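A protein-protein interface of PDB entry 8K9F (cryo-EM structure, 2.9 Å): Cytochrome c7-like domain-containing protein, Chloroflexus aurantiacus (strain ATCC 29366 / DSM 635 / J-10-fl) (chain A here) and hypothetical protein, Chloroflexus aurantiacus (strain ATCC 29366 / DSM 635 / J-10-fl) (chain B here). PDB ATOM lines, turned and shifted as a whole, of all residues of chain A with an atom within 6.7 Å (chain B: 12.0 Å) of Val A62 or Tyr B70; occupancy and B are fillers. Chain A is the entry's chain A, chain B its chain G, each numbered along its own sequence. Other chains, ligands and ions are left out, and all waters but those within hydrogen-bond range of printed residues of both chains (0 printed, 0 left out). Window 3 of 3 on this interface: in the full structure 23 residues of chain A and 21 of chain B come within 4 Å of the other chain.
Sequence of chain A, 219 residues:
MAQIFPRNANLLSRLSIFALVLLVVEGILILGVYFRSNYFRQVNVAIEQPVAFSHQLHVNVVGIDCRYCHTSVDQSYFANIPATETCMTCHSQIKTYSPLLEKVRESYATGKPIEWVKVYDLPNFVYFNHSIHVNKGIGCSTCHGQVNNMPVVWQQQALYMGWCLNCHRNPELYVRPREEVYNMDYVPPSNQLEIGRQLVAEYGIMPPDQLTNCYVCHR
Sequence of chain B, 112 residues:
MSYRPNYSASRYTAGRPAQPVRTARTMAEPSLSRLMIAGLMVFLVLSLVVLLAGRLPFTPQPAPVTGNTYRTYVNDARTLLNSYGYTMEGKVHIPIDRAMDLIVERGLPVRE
Of the 15 printed residues of chain A, 7 touch a printed residue of chain B.
Printed residues of chain A that touch a printed residue of chain B: Gln A56, Val A59, Asn A60, Val A61, Val A62, Gly A63 and Asn A183.
Hydrophobic or aromatic side chains of chain A within 4 Å of the printed part of chain B: Val A61.
Hydrophobic or aromatic side chains of chain B within 4 Å of the printed part of chain A: Val B65 and Tyr B70.
Among the printed residues, 12 pairs touch across the chains.
Among the printed residues, no Asp or Glu carboxylate lies within 4 Å of a Lys or Arg side-chain nitrogen of the other chain.
The backbone carbonyl oxygen (O) of Asn A60 lies close to the side-chain hydroxyl (OG1) of Thr B69 (2.3 Å).
The side-chain amide oxygen (OD1) of Asn A60 sits at hydrogen-bond distance from the guanidinium group (NH2) of Arg B71, 2.7 Å away.
The backbone carbonyl oxygen (O) of Val A61 is in hydrogen-bond range of the backbone NH (N) of Tyr B70 (2.8 Å).
OH of Tyr B70 lies within hydrogen-bond range of ND2 of Asn A183 (2.7 Å).
Among the printed residues, merely in contact across the chains: Gln A56 with Val B65, Val A59 with Tyr B70, Asn A60 with Tyr B70, Val A61 with Val B65, Val A61 with Asn B68, Val A61 with Thr B69, Val A62 with Tyr B70 and Gly A63 with Tyr B70.
O of Arg B71 lies within hydrogen-bond range of ND2 of Asn B75 (2.8 Å).
ND2 of Asn A60 is in hydrogen-bond range of O of Asn A148 (2.9 Å).
OG1 of Thr B69 is in hydrogen-bond range of NH1 of Arg B71, 3.3 Å away.
OD1 of Asn A183 lies within hydrogen-bond range of ND2 of Asn A148, 2.5 Å away.
The backbone carbonyl oxygen of Gln A56 lies close to the backbone NH of Val A61, 3.4 Å away.
The backbone carbonyl oxygen (O) of Leu A57 is in hydrogen-bond range of the backbone NH (N) of Val A62, at 2.8 Å.
No residue of chain B comes within 4 Å of Leu A57.
No residue of chain B comes within 4 Å of His A58.
Val A59 touches just one residue of chain B: Tyr B70 (3.4 Å).
Printed residues of chain B within 4 Å of Asn A60: Thr B69 (2.3 Å), Tyr B70 (3.2 Å) and Arg B71 (2.7 Å).
No residue of chain B comes within 4 Å of Ile A64.
Printed residues of chain A within 4 Å of Val B65: Gln A56 (3.99 Å) and Val A61 (3.7 Å).
Thr B66 touches none of the printed residues of chain A.
Of the printed residues of chain A, Asn B68 touches Val A61.
Of chain A, only Val A59 (3.4 Å), Asn A60 (3.2 Å), Val A61 (2.8 Å), Val A62 (3.4 Å), Gly A63 (3.5 Å) and Asn A183 (2.7 Å) come within 4 Å of Tyr B70.
Thr B79 touches none of the printed residues of chain A.
The nearest printed residue of chain A that does not touch Thr B69 is Val A62 (5.2 Å).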
ATOM      1  N   GLN A  56      21.563 -13.197   7.571  1.00  0.00           N
ATOM      2  CA  GLN A  56      21.890 -14.492   8.169  1.00  0.00           C
ATOM      3  C   GLN A  56      20.654 -15.349   8.362  1.00  0.00           C
ATOM      4  O   GLN A  56      20.711 -16.573   8.210  1.00  0.00           O
ATOM      5  CB  GLN A  56      22.604 -14.309   9.507  1.00  0.00           C
ATOM      6  CG  GLN A  56      23.247 -15.582  10.014  1.00  0.00           C
ATOM      7  CD  GLN A  56      23.806 -15.442  11.397  1.00  0.00           C
ATOM      8  OE1 GLN A  56      25.019 -15.371  11.572  1.00  0.00           O
ATOM      9  NE2 GLN A  56      22.933 -15.411  12.394  1.00  0.00           N
ATOM     10  N   LEU A  57      19.530 -14.724   8.688  1.00  0.00           N
ATOM     11  CA  LEU A  57      18.330 -15.483   8.993  1.00  0.00           C
ATOM     12  C   LEU A  57      17.570 -15.809   7.715  1.00  0.00           C
ATOM     13  O   LEU A  57      16.877 -16.824   7.637  1.00  0.00           O
ATOM     14  CB  LEU A  57      17.434 -14.712   9.964  1.00  0.00           C
ATOM     15  CG  LEU A  57      16.096 -15.367  10.317  1.00  0.00           C
ATOM     16  CD1 LEU A  57      16.320 -16.690  11.036  1.00  0.00           C
ATOM     17  CD2 LEU A  57      15.244 -14.432  11.161  1.00  0.00           C
ATOM     18  N   HIS A  58      17.699 -14.974   6.696  1.00  0.00           N
ATOM     19  CA  HIS A  58      16.917 -15.196   5.491  1.00  0.00           C
ATOM     20  C   HIS A  58      17.618 -16.109   4.504  1.00  0.00           C
ATOM     21  O   HIS A  58      16.969 -16.948   3.881  1.00  0.00           O
ATOM     22  CB  HIS A  58      16.592 -13.858   4.835  1.00  0.00           C
ATOM     23  CG  HIS A  58      15.477 -13.128   5.503  1.00  0.00           C
ATOM     24  ND1 HIS A  58      15.700 -12.177   6.471  1.00  0.00           N
ATOM     25  CD2 HIS A  58      14.135 -13.200   5.347  1.00  0.00           C
ATOM     26  CE1 HIS A  58      14.542 -11.703   6.893  1.00  0.00           C
ATOM     27  NE2 HIS A  58      13.573 -12.301   6.224  1.00  0.00           N
ATOM     28  N   VAL A  59      18.929 -15.992   4.349  1.00  0.00           N
ATOM     29  CA  VAL A  59      19.613 -16.707   3.290  1.00  0.00           C
ATOM     30  C   VAL A  59      20.235 -17.995   3.806  1.00  0.00           C
ATOM     31  O   VAL A  59      20.061 -19.059   3.213  1.00  0.00           O
ATOM     32  CB  VAL A  59      20.662 -15.789   2.629  1.00  0.00           C
ATOM     33  CG1 VAL A  59      21.511 -16.573   1.669  1.00  0.00           C
ATOM     34  CG2 VAL A  59      19.990 -14.620   1.959  1.00  0.00           C
ATOM     35  N   ASN A  60      20.959 -17.930   4.922  1.00  0.00           N
ATOM     36  CA  ASN A  60      21.535 -19.149   5.476  1.00  0.00           C
ATOM     37  C   ASN A  60      20.506 -20.016   6.168  1.00  0.00           C
ATOM     38  O   ASN A  60      20.662 -21.238   6.185  1.00  0.00           O
ATOM     39  CB  ASN A  60      22.649 -18.829   6.465  1.00  0.00           C
ATOM     40  CG  ASN A  60      24.019 -18.934   5.842  1.00  0.00           C
ATOM     41  OD1 ASN A  60      24.165 -19.421   4.724  1.00  0.00           O
ATOM     42  ND2 ASN A  60      25.029 -18.455   6.551  1.00  0.00           N
ATOM     43  N   VAL A  61      19.459 -19.424   6.728  1.00  0.00           N
ATOM     44  CA  VAL A  61      18.472 -20.160   7.503  1.00  0.00           C
ATOM     45  C   VAL A  61      17.180 -20.349   6.715  1.00  0.00           C
ATOM     46  O   VAL A  61      16.865 -21.465   6.307  1.00  0.00           O
ATOM     47  CB  VAL A  61      18.226 -19.480   8.868  1.00  0.00           C
ATOM     48  CG1 VAL A  61      17.343 -20.294   9.750  1.00  0.00           C
ATOM     49  CG2 VAL A  61      19.536 -19.294   9.563  1.00  0.00           C
ATOM     50  N   VAL A  62      16.471 -19.259   6.403  1.00  0.00           N
ATOM     51  CA  VAL A  62      15.198 -19.392   5.689  1.00  0.00           C
ATOM     52  C   VAL A  62      15.442 -19.824   4.243  1.00  0.00           C
ATOM     53  O   VAL A  62      14.752 -20.704   3.715  1.00  0.00           O
ATOM     54  CB  VAL A  62      14.389 -18.085   5.792  1.00  0.00           C
ATOM     55  CG1 VAL A  62      13.348 -17.980   4.702  1.00  0.00           C
ATOM     56  CG2 VAL A  62      13.719 -17.995   7.152  1.00  0.00           C
ATOM     57  N   GLY A  63      16.459 -19.262   3.607  1.00  0.00           N
ATOM     58  CA  GLY A  63      16.990 -19.849   2.396  1.00  0.00           C
ATOM     59  C   GLY A  63      16.466 -19.285   1.100  1.00  0.00           C
ATOM     60  O   GLY A  63      16.138 -20.048   0.188  1.00  0.00           O
ATOM     61  N   ILE A  64      16.394 -17.978   0.977  1.00  0.00           N
ATOM     62  CA  ILE A  64      15.939 -17.419  -0.282  1.00  0.00           C
ATOM     63  C   ILE A  64      17.170 -17.049  -1.090  1.00  0.00           C
ATOM     64  O   ILE A  64      18.152 -16.537  -0.543  1.00  0.00           O
ATOM     65  CB  ILE A  64      15.019 -16.197  -0.110  1.00  0.00           C
ATOM     66  CG1 ILE A  64      14.079 -16.295   1.075  1.00  0.00           C
ATOM     67  CG2 ILE A  64      14.058 -16.193  -1.214  1.00  0.00           C
ATOM     68  CD1 ILE A  64      14.548 -15.550   2.259  1.00  0.00           C
ATOM     69  N   CYS A  90       5.698 -12.762   2.135  1.00  0.00           N
ATOM     70  CA  CYS A  90       5.854 -13.585   3.320  1.00  0.00           C
ATOM     71  C   CYS A  90       5.225 -12.916   4.537  1.00  0.00           C
ATOM     72  O   CYS A  90       4.505 -13.560   5.302  1.00  0.00           O
ATOM     73  CB  CYS A  90       7.340 -13.851   3.558  1.00  0.00           C
ATOM     74  SG  CYS A  90       8.035 -15.389   2.897  1.00  0.00           S
ATOM     75  N   ASN A 148      25.560 -14.128   3.368  1.00  0.00           N
ATOM     76  CA  ASN A 148      24.619 -15.124   3.855  1.00  0.00           C
ATOM     77  C   ASN A 148      24.731 -15.383   5.349  1.00  0.00           C
ATOM     78  O   ASN A 148      23.773 -15.872   5.940  1.00  0.00           O
ATOM     79  CB  ASN A 148      24.807 -16.433   3.093  1.00  0.00           C
ATOM     80  CG  ASN A 148      26.173 -17.032   3.274  1.00  0.00           C
ATOM     81  OD1 ASN A 148      27.127 -16.344   3.629  1.00  0.00           O
ATOM     82  ND2 ASN A 148      26.284 -18.328   3.005  1.00  0.00           N
ATOM     83  N   TYR A 182      25.222 -18.455  -6.660  1.00  0.00           N
ATOM     84  CA  TYR A 182      25.219 -19.528  -5.688  1.00  0.00           C
ATOM     85  C   TYR A 182      25.551 -18.966  -4.317  1.00  0.00           C
ATOM     86  O   TYR A 182      26.270 -17.971  -4.194  1.00  0.00           O
ATOM     87  CB  TYR A 182      26.227 -20.606  -6.095  1.00  0.00           C
ATOM     88  CG  TYR A 182      26.386 -21.728  -5.099  1.00  0.00           C
ATOM     89  CD1 TYR A 182      25.296 -22.506  -4.718  1.00  0.00           C
ATOM     90  CD2 TYR A 182      27.622 -22.011  -4.536  1.00  0.00           C
ATOM     91  CE1 TYR A 182      25.435 -23.531  -3.797  1.00  0.00           C
ATOM     92  CE2 TYR A 182      27.772 -23.030  -3.615  1.00  0.00           C
ATOM     93  CZ  TYR A 182      26.675 -23.788  -3.253  1.00  0.00           C
ATOM     94  OH  TYR A 182      26.818 -24.806  -2.338  1.00  0.00           O
ATOM     95  N   ASN A 183      24.966 -19.592  -3.293  1.00  0.00           N
ATOM     96  CA  ASN A 183      25.169 -19.251  -1.893  1.00  0.00           C
ATOM     97  C   ASN A 183      26.652 -19.281  -1.539  1.00  0.00           C
ATOM     98  O   ASN A 183      27.464 -19.947  -2.183  1.00  0.00           O
ATOM     99  CB  ASN A 183      24.394 -20.235  -1.007  1.00  0.00           C
ATOM    100  CG  ASN A 183      24.084 -19.682   0.379  1.00  0.00           C
ATOM    101  OD1 ASN A 183      24.922 -19.041   1.012  1.00  0.00           O
ATOM    102  ND2 ASN A 183      22.872 -19.934   0.853  1.00  0.00           N
ATOM    103  N   MET A 184      27.010 -18.575  -0.473  1.00  0.00           N
ATOM    104  CA  MET A 184      28.404 -18.531  -0.039  1.00  0.00           C
ATOM    105  C   MET A 184      28.791 -19.793   0.747  1.00  0.00           C
ATOM    106  O   MET A 184      29.222 -19.757   1.897  1.00  0.00           O
ATOM    107  CB  MET A 184      28.664 -17.260   0.758  1.00  0.00           C
ATOM    108  CG  MET A 184      27.813 -16.048   0.367  1.00  0.00           C
ATOM    109  SD  MET A 184      27.840 -15.660  -1.395  1.00  0.00           S
ATOM    110  CE  MET A 184      26.117 -15.626  -1.802  1.00  0.00           C
ATOM    111  N   ASP A 185      28.606 -20.933   0.083  1.00  0.00           N
ATOM    112  CA  ASP A 185      29.254 -22.185   0.414  1.00  0.00           C
ATOM    113  C   ASP A 185      30.386 -22.485  -0.557  1.00  0.00           C
ATOM    114  O   ASP A 185      31.074 -23.500  -0.403  1.00  0.00           O
ATOM    115  CB  ASP A 185      28.227 -23.325   0.408  1.00  0.00           C
ATOM    116  CG  ASP A 185      28.647 -24.499   1.272  1.00  0.00           C
ATOM    117  OD1 ASP A 185      29.543 -24.321   2.124  1.00  0.00           O
ATOM    118  OD2 ASP A 185      28.082 -25.600   1.100  1.00  0.00           O
ATOM    119  N   VAL B  65      24.843 -19.733  13.515  1.00  0.00           N
ATOM    120  CA  VAL B  65      23.418 -19.956  13.702  1.00  0.00           C
ATOM    121  C   VAL B  65      23.158 -21.418  14.056  1.00  0.00           C
ATOM    122  O   VAL B  65      23.983 -22.310  13.823  1.00  0.00           O
ATOM    123  CB  VAL B  65      22.640 -19.520  12.446  1.00  0.00           C
ATOM    124  CG1 VAL B  65      22.586 -20.630  11.400  1.00  0.00           C
ATOM    125  CG2 VAL B  65      21.253 -19.009  12.811  1.00  0.00           C
ATOM    126  N   THR B  66      22.010 -21.656  14.681  1.00  0.00           N
ATOM    127  CA  THR B  66      21.595 -22.998  15.041  1.00  0.00           C
ATOM    128  C   THR B  66      20.127 -23.164  14.682  1.00  0.00           C
ATOM    129  O   THR B  66      19.526 -22.312  14.021  1.00  0.00           O
ATOM    130  CB  THR B  66      21.830 -23.287  16.525  1.00  0.00           C
ATOM    131  OG1 THR B  66      21.266 -24.562  16.851  1.00  0.00           O
ATOM    132  CG2 THR B  66      21.180 -22.211  17.384  1.00  0.00           C
ATOM    133  N   GLY B  67      19.550 -24.270  15.130  1.00  0.00           N
ATOM    134  CA  GLY B  67      18.251 -24.689  14.654  1.00  0.00           C
ATOM    135  C   GLY B  67      18.348 -25.342  13.287  1.00  0.00           C
ATOM    136  O   GLY B  67      19.423 -25.497  12.711  1.00  0.00           O
ATOM    137  N   ASN B  68      17.194 -25.746  12.768  1.00  0.00           N
ATOM    138  CA  ASN B  68      17.166 -26.265  11.410  1.00  0.00           C
ATOM    139  C   ASN B  68      17.373 -25.136  10.410  1.00  0.00           C
ATOM    140  O   ASN B  68      17.071 -23.973  10.689  1.00  0.00           O
ATOM    141  CB  ASN B  68      15.874 -27.077  11.161  1.00  0.00           C
ATOM    142  CG  ASN B  68      15.811 -28.434  11.894  1.00  0.00           C
ATOM    143  OD1 ASN B  68      16.821 -29.037  12.270  1.00  0.00           O
ATOM    144  ND2 ASN B  68      14.587 -28.904  12.111  1.00  0.00           N
ATOM    145  N   THR B  69      17.949 -25.470   9.272  1.00  0.00           N
ATOM    146  CA  THR B  69      18.156 -24.523   8.197  1.00  0.00           C
ATOM    147  C   THR B  69      17.422 -25.015   6.955  1.00  0.00           C
ATOM    148  O   THR B  69      16.817 -26.088   6.947  1.00  0.00           O
ATOM    149  CB  THR B  69      19.650 -24.313   7.948  1.00  0.00           C
ATOM    150  OG1 THR B  69      19.844 -23.212   7.055  1.00  0.00           O
ATOM    151  CG2 THR B  69      20.274 -25.557   7.370  1.00  0.00           C
ATOM    152  N   TYR B  70      17.463 -24.200   5.902  1.00  0.00           N
ATOM    153  CA  TYR B  70      16.854 -24.576   4.634  1.00  0.00           C
ATOM    154  C   TYR B  70      17.578 -25.715   3.941  1.00  0.00           C
ATOM    155  O   TYR B  70      16.986 -26.348   3.064  1.00  0.00           O
ATOM    156  CB  TYR B  70      16.804 -23.379   3.683  1.00  0.00           C
ATOM    157  CG  TYR B  70      18.111 -23.096   2.969  1.00  0.00           C
ATOM    158  CD1 TYR B  70      19.246 -22.720   3.676  1.00  0.00           C
ATOM    159  CD2 TYR B  70      18.209 -23.210   1.590  1.00  0.00           C
ATOM    160  CE1 TYR B  70      20.431 -22.457   3.037  1.00  0.00           C
ATOM    161  CE2 TYR B  70      19.400 -22.959   0.939  1.00  0.00           C
ATOM    162  CZ  TYR B  70      20.508 -22.583   1.671  1.00  0.00           C
ATOM    163  OH  TYR B  70      21.697 -22.326   1.034  1.00  0.00           O
ATOM    164  N   ARG B  71      18.836 -25.981   4.310  1.00  0.00           N
ATOM    165  CA  ARG B  71      19.662 -26.930   3.572  1.00  0.00           C
ATOM    166  C   ARG B  71      19.157 -28.356   3.679  1.00  0.00           C
ATOM    167  O   ARG B  71      19.310 -29.113   2.722  1.00  0.00           O
ATOM    168  CB  ARG B  71      21.111 -26.869   4.046  1.00  0.00           C
ATOM    169  CG  ARG B  71      21.867 -25.670   3.551  1.00  0.00           C
ATOM    170  CD  ARG B  71      23.185 -25.514   4.260  1.00  0.00           C
ATOM    171  NE  ARG B  71      23.828 -24.256   3.906  1.00  0.00           N
ATOM    172  CZ  ARG B  71      23.599 -23.105   4.518  1.00  0.00           C
ATOM    173  NH1 ARG B  71      22.739 -23.014   5.518  1.00  0.00           N
ATOM    174  NH2 ARG B  71      24.248 -22.015   4.116  1.00  0.00           N
ATOM    175  N   THR B  72      18.556 -28.734   4.813  1.00  0.00           N
ATOM    176  CA  THR B  72      18.080 -30.106   4.991  1.00  0.00           C
ATOM    177  C   THR B  72      16.957 -30.429   4.011  1.00  0.00           C
ATOM    178  O   THR B  72      17.029 -31.421   3.269  1.00  0.00           O
ATOM    179  CB  THR B  72      17.624 -30.311   6.437  1.00  0.00           C
ATOM    180  OG1 THR B  72      18.773 -30.481   7.278  1.00  0.00           O
ATOM    181  CG2 THR B  72      16.738 -31.551   6.570  1.00  0.00           C
ATOM    182  N   TYR B  73      15.939 -29.561   3.952  1.00  0.00           N
ATOM    183  CA  TYR B  73      14.862 -29.710   2.978  1.00  0.00           C
ATOM    184  C   TYR B  73      15.370 -29.581   1.554  1.00  0.00           C
ATOM    185  O   TYR B  73      14.885 -30.287   0.662  1.00  0.00           O
ATOM    186  CB  TYR B  73      13.771 -28.666   3.221  1.00  0.00           C
ATOM    187  CG  TYR B  73      13.071 -28.771   4.552  1.00  0.00           C
ATOM    188  CD1 TYR B  73      12.559 -29.984   4.999  1.00  0.00           C
ATOM    189  CD2 TYR B  73      12.911 -27.655   5.359  1.00  0.00           C
ATOM    190  CE1 TYR B  73      11.911 -30.082   6.215  1.00  0.00           C
ATOM    191  CE2 TYR B  73      12.263 -27.742   6.574  1.00  0.00           C
ATOM    192  CZ  TYR B  73      11.768 -28.956   6.998  1.00  0.00           C
ATOM    193  OH  TYR B  73      11.126 -29.036   8.212  1.00  0.00           O
ATOM    194  N   VAL B  74      16.352 -28.703   1.328  1.00  0.00           N
ATOM    195  CA  VAL B  74      16.839 -28.443  -0.025  1.00  0.00           C
ATOM    196  C   VAL B  74      17.570 -29.662  -0.573  1.00  0.00           C
ATOM    197  O   VAL B  74      17.287 -30.107  -1.688  1.00  0.00           O
ATOM    198  CB  VAL B  74      17.713 -27.174  -0.058  1.00  0.00           C
ATOM    199  CG1 VAL B  74      18.767 -27.226  -1.158  1.00  0.00           C
ATOM    200  CG2 VAL B  74      16.835 -25.962  -0.276  1.00  0.00           C
ATOM    201  N   ASN B  75      18.477 -30.259   0.210  1.00  0.00           N
ATOM    202  CA  ASN B  75      19.169 -31.422  -0.331  1.00  0.00           C
ATOM    203  C   ASN B  75      18.307 -32.677  -0.274  1.00  0.00           C
ATOM    204  O   ASN B  75      18.533 -33.591  -1.075  1.00  0.00           O
ATOM    205  CB  ASN B  75      20.531 -31.656   0.349  1.00  0.00           C
ATOM    206  CG  ASN B  75      20.459 -31.740   1.864  1.00  0.00           C
ATOM    207  OD1 ASN B  75      19.617 -32.423   2.442  1.00  0.00           O
ATOM    208  ND2 ASN B  75      21.358 -31.020   2.519  1.00  0.00           N
ATOM    209  N   ASP B  76      17.303 -32.727   0.612  1.00  0.00           N
ATOM    210  CA  ASP B  76      16.328 -33.813   0.551  1.00  0.00           C
ATOM    211  C   ASP B  76      15.529 -33.763  -0.746  1.00  0.00           C
ATOM    212  O   ASP B  76      15.362 -34.785  -1.421  1.00  0.00           O
ATOM    213  CB  ASP B  76      15.396 -33.751   1.759  1.00  0.00           C
ATOM    214  CG  ASP B  76      15.717 -34.808   2.798  1.00  0.00           C
ATOM    215  OD1 ASP B  76      16.580 -35.668   2.528  1.00  0.00           O
ATOM    216  OD2 ASP B  76      15.107 -34.775   3.887  1.00  0.00           O
ATOM    217  N   ALA B  77      15.070 -32.574  -1.142  1.00  0.00           N
ATOM    218  CA  ALA B  77      14.363 -32.441  -2.410  1.00  0.00           C
ATOM    219  C   ALA B  77      15.296 -32.563  -3.608  1.00  0.00           C
ATOM    220  O   ALA B  77      14.853 -32.966  -4.685  1.00  0.00           O
ATOM    221  CB  ALA B  77      13.619 -31.110  -2.463  1.00  0.00           C
ATOM    222  N   ARG B  78      16.575 -32.218  -3.450  1.00  0.00           N
ATOM    223  CA  ARG B  78      17.531 -32.408  -4.535  1.00  0.00           C
ATOM    224  C   ARG B  78      17.822 -33.881  -4.758  1.00  0.00           C
ATOM    225  O   ARG B  78      18.075 -34.299  -5.893  1.00  0.00           O
ATOM    226  CB  ARG B  78      18.828 -31.652  -4.245  1.00  0.00           C
ATOM    227  CG  ARG B  78      18.773 -30.173  -4.570  1.00  0.00           C
ATOM    228  CD  ARG B  78      20.163 -29.609  -4.847  1.00  0.00           C
ATOM    229  NE  ARG B  78      20.383 -28.314  -4.209  1.00  0.00           N
ATOM    230  CZ  ARG B  78      19.926 -27.154  -4.665  1.00  0.00           C
ATOM    231  NH1 ARG B  78      19.187 -27.082  -5.760  1.00  0.00           N
ATOM    232  NH2 ARG B  78      20.221 -26.038  -4.008  1.00  0.00           N
ATOM    233  N   THR B  79      17.820 -34.674  -3.685  1.00  0.00           N
ATOM    234  CA  THR B  79      17.814 -36.124  -3.830  1.00  0.00           C
ATOM    235  C   THR B  79      16.514 -36.601  -4.467  1.00  0.00           C
ATOM    236  O   THR B  79      16.530 -37.452  -5.361  1.00  0.00           O
ATOM    237  CB  THR B  79      18.023 -36.775  -2.462  1.00  0.00           C
ATOM    238  OG1 THR B  79      19.273 -36.337  -1.915  1.00  0.00           O
ATOM    239  CG2 THR B  79      18.024 -38.290  -2.565  1.00  0.00           C
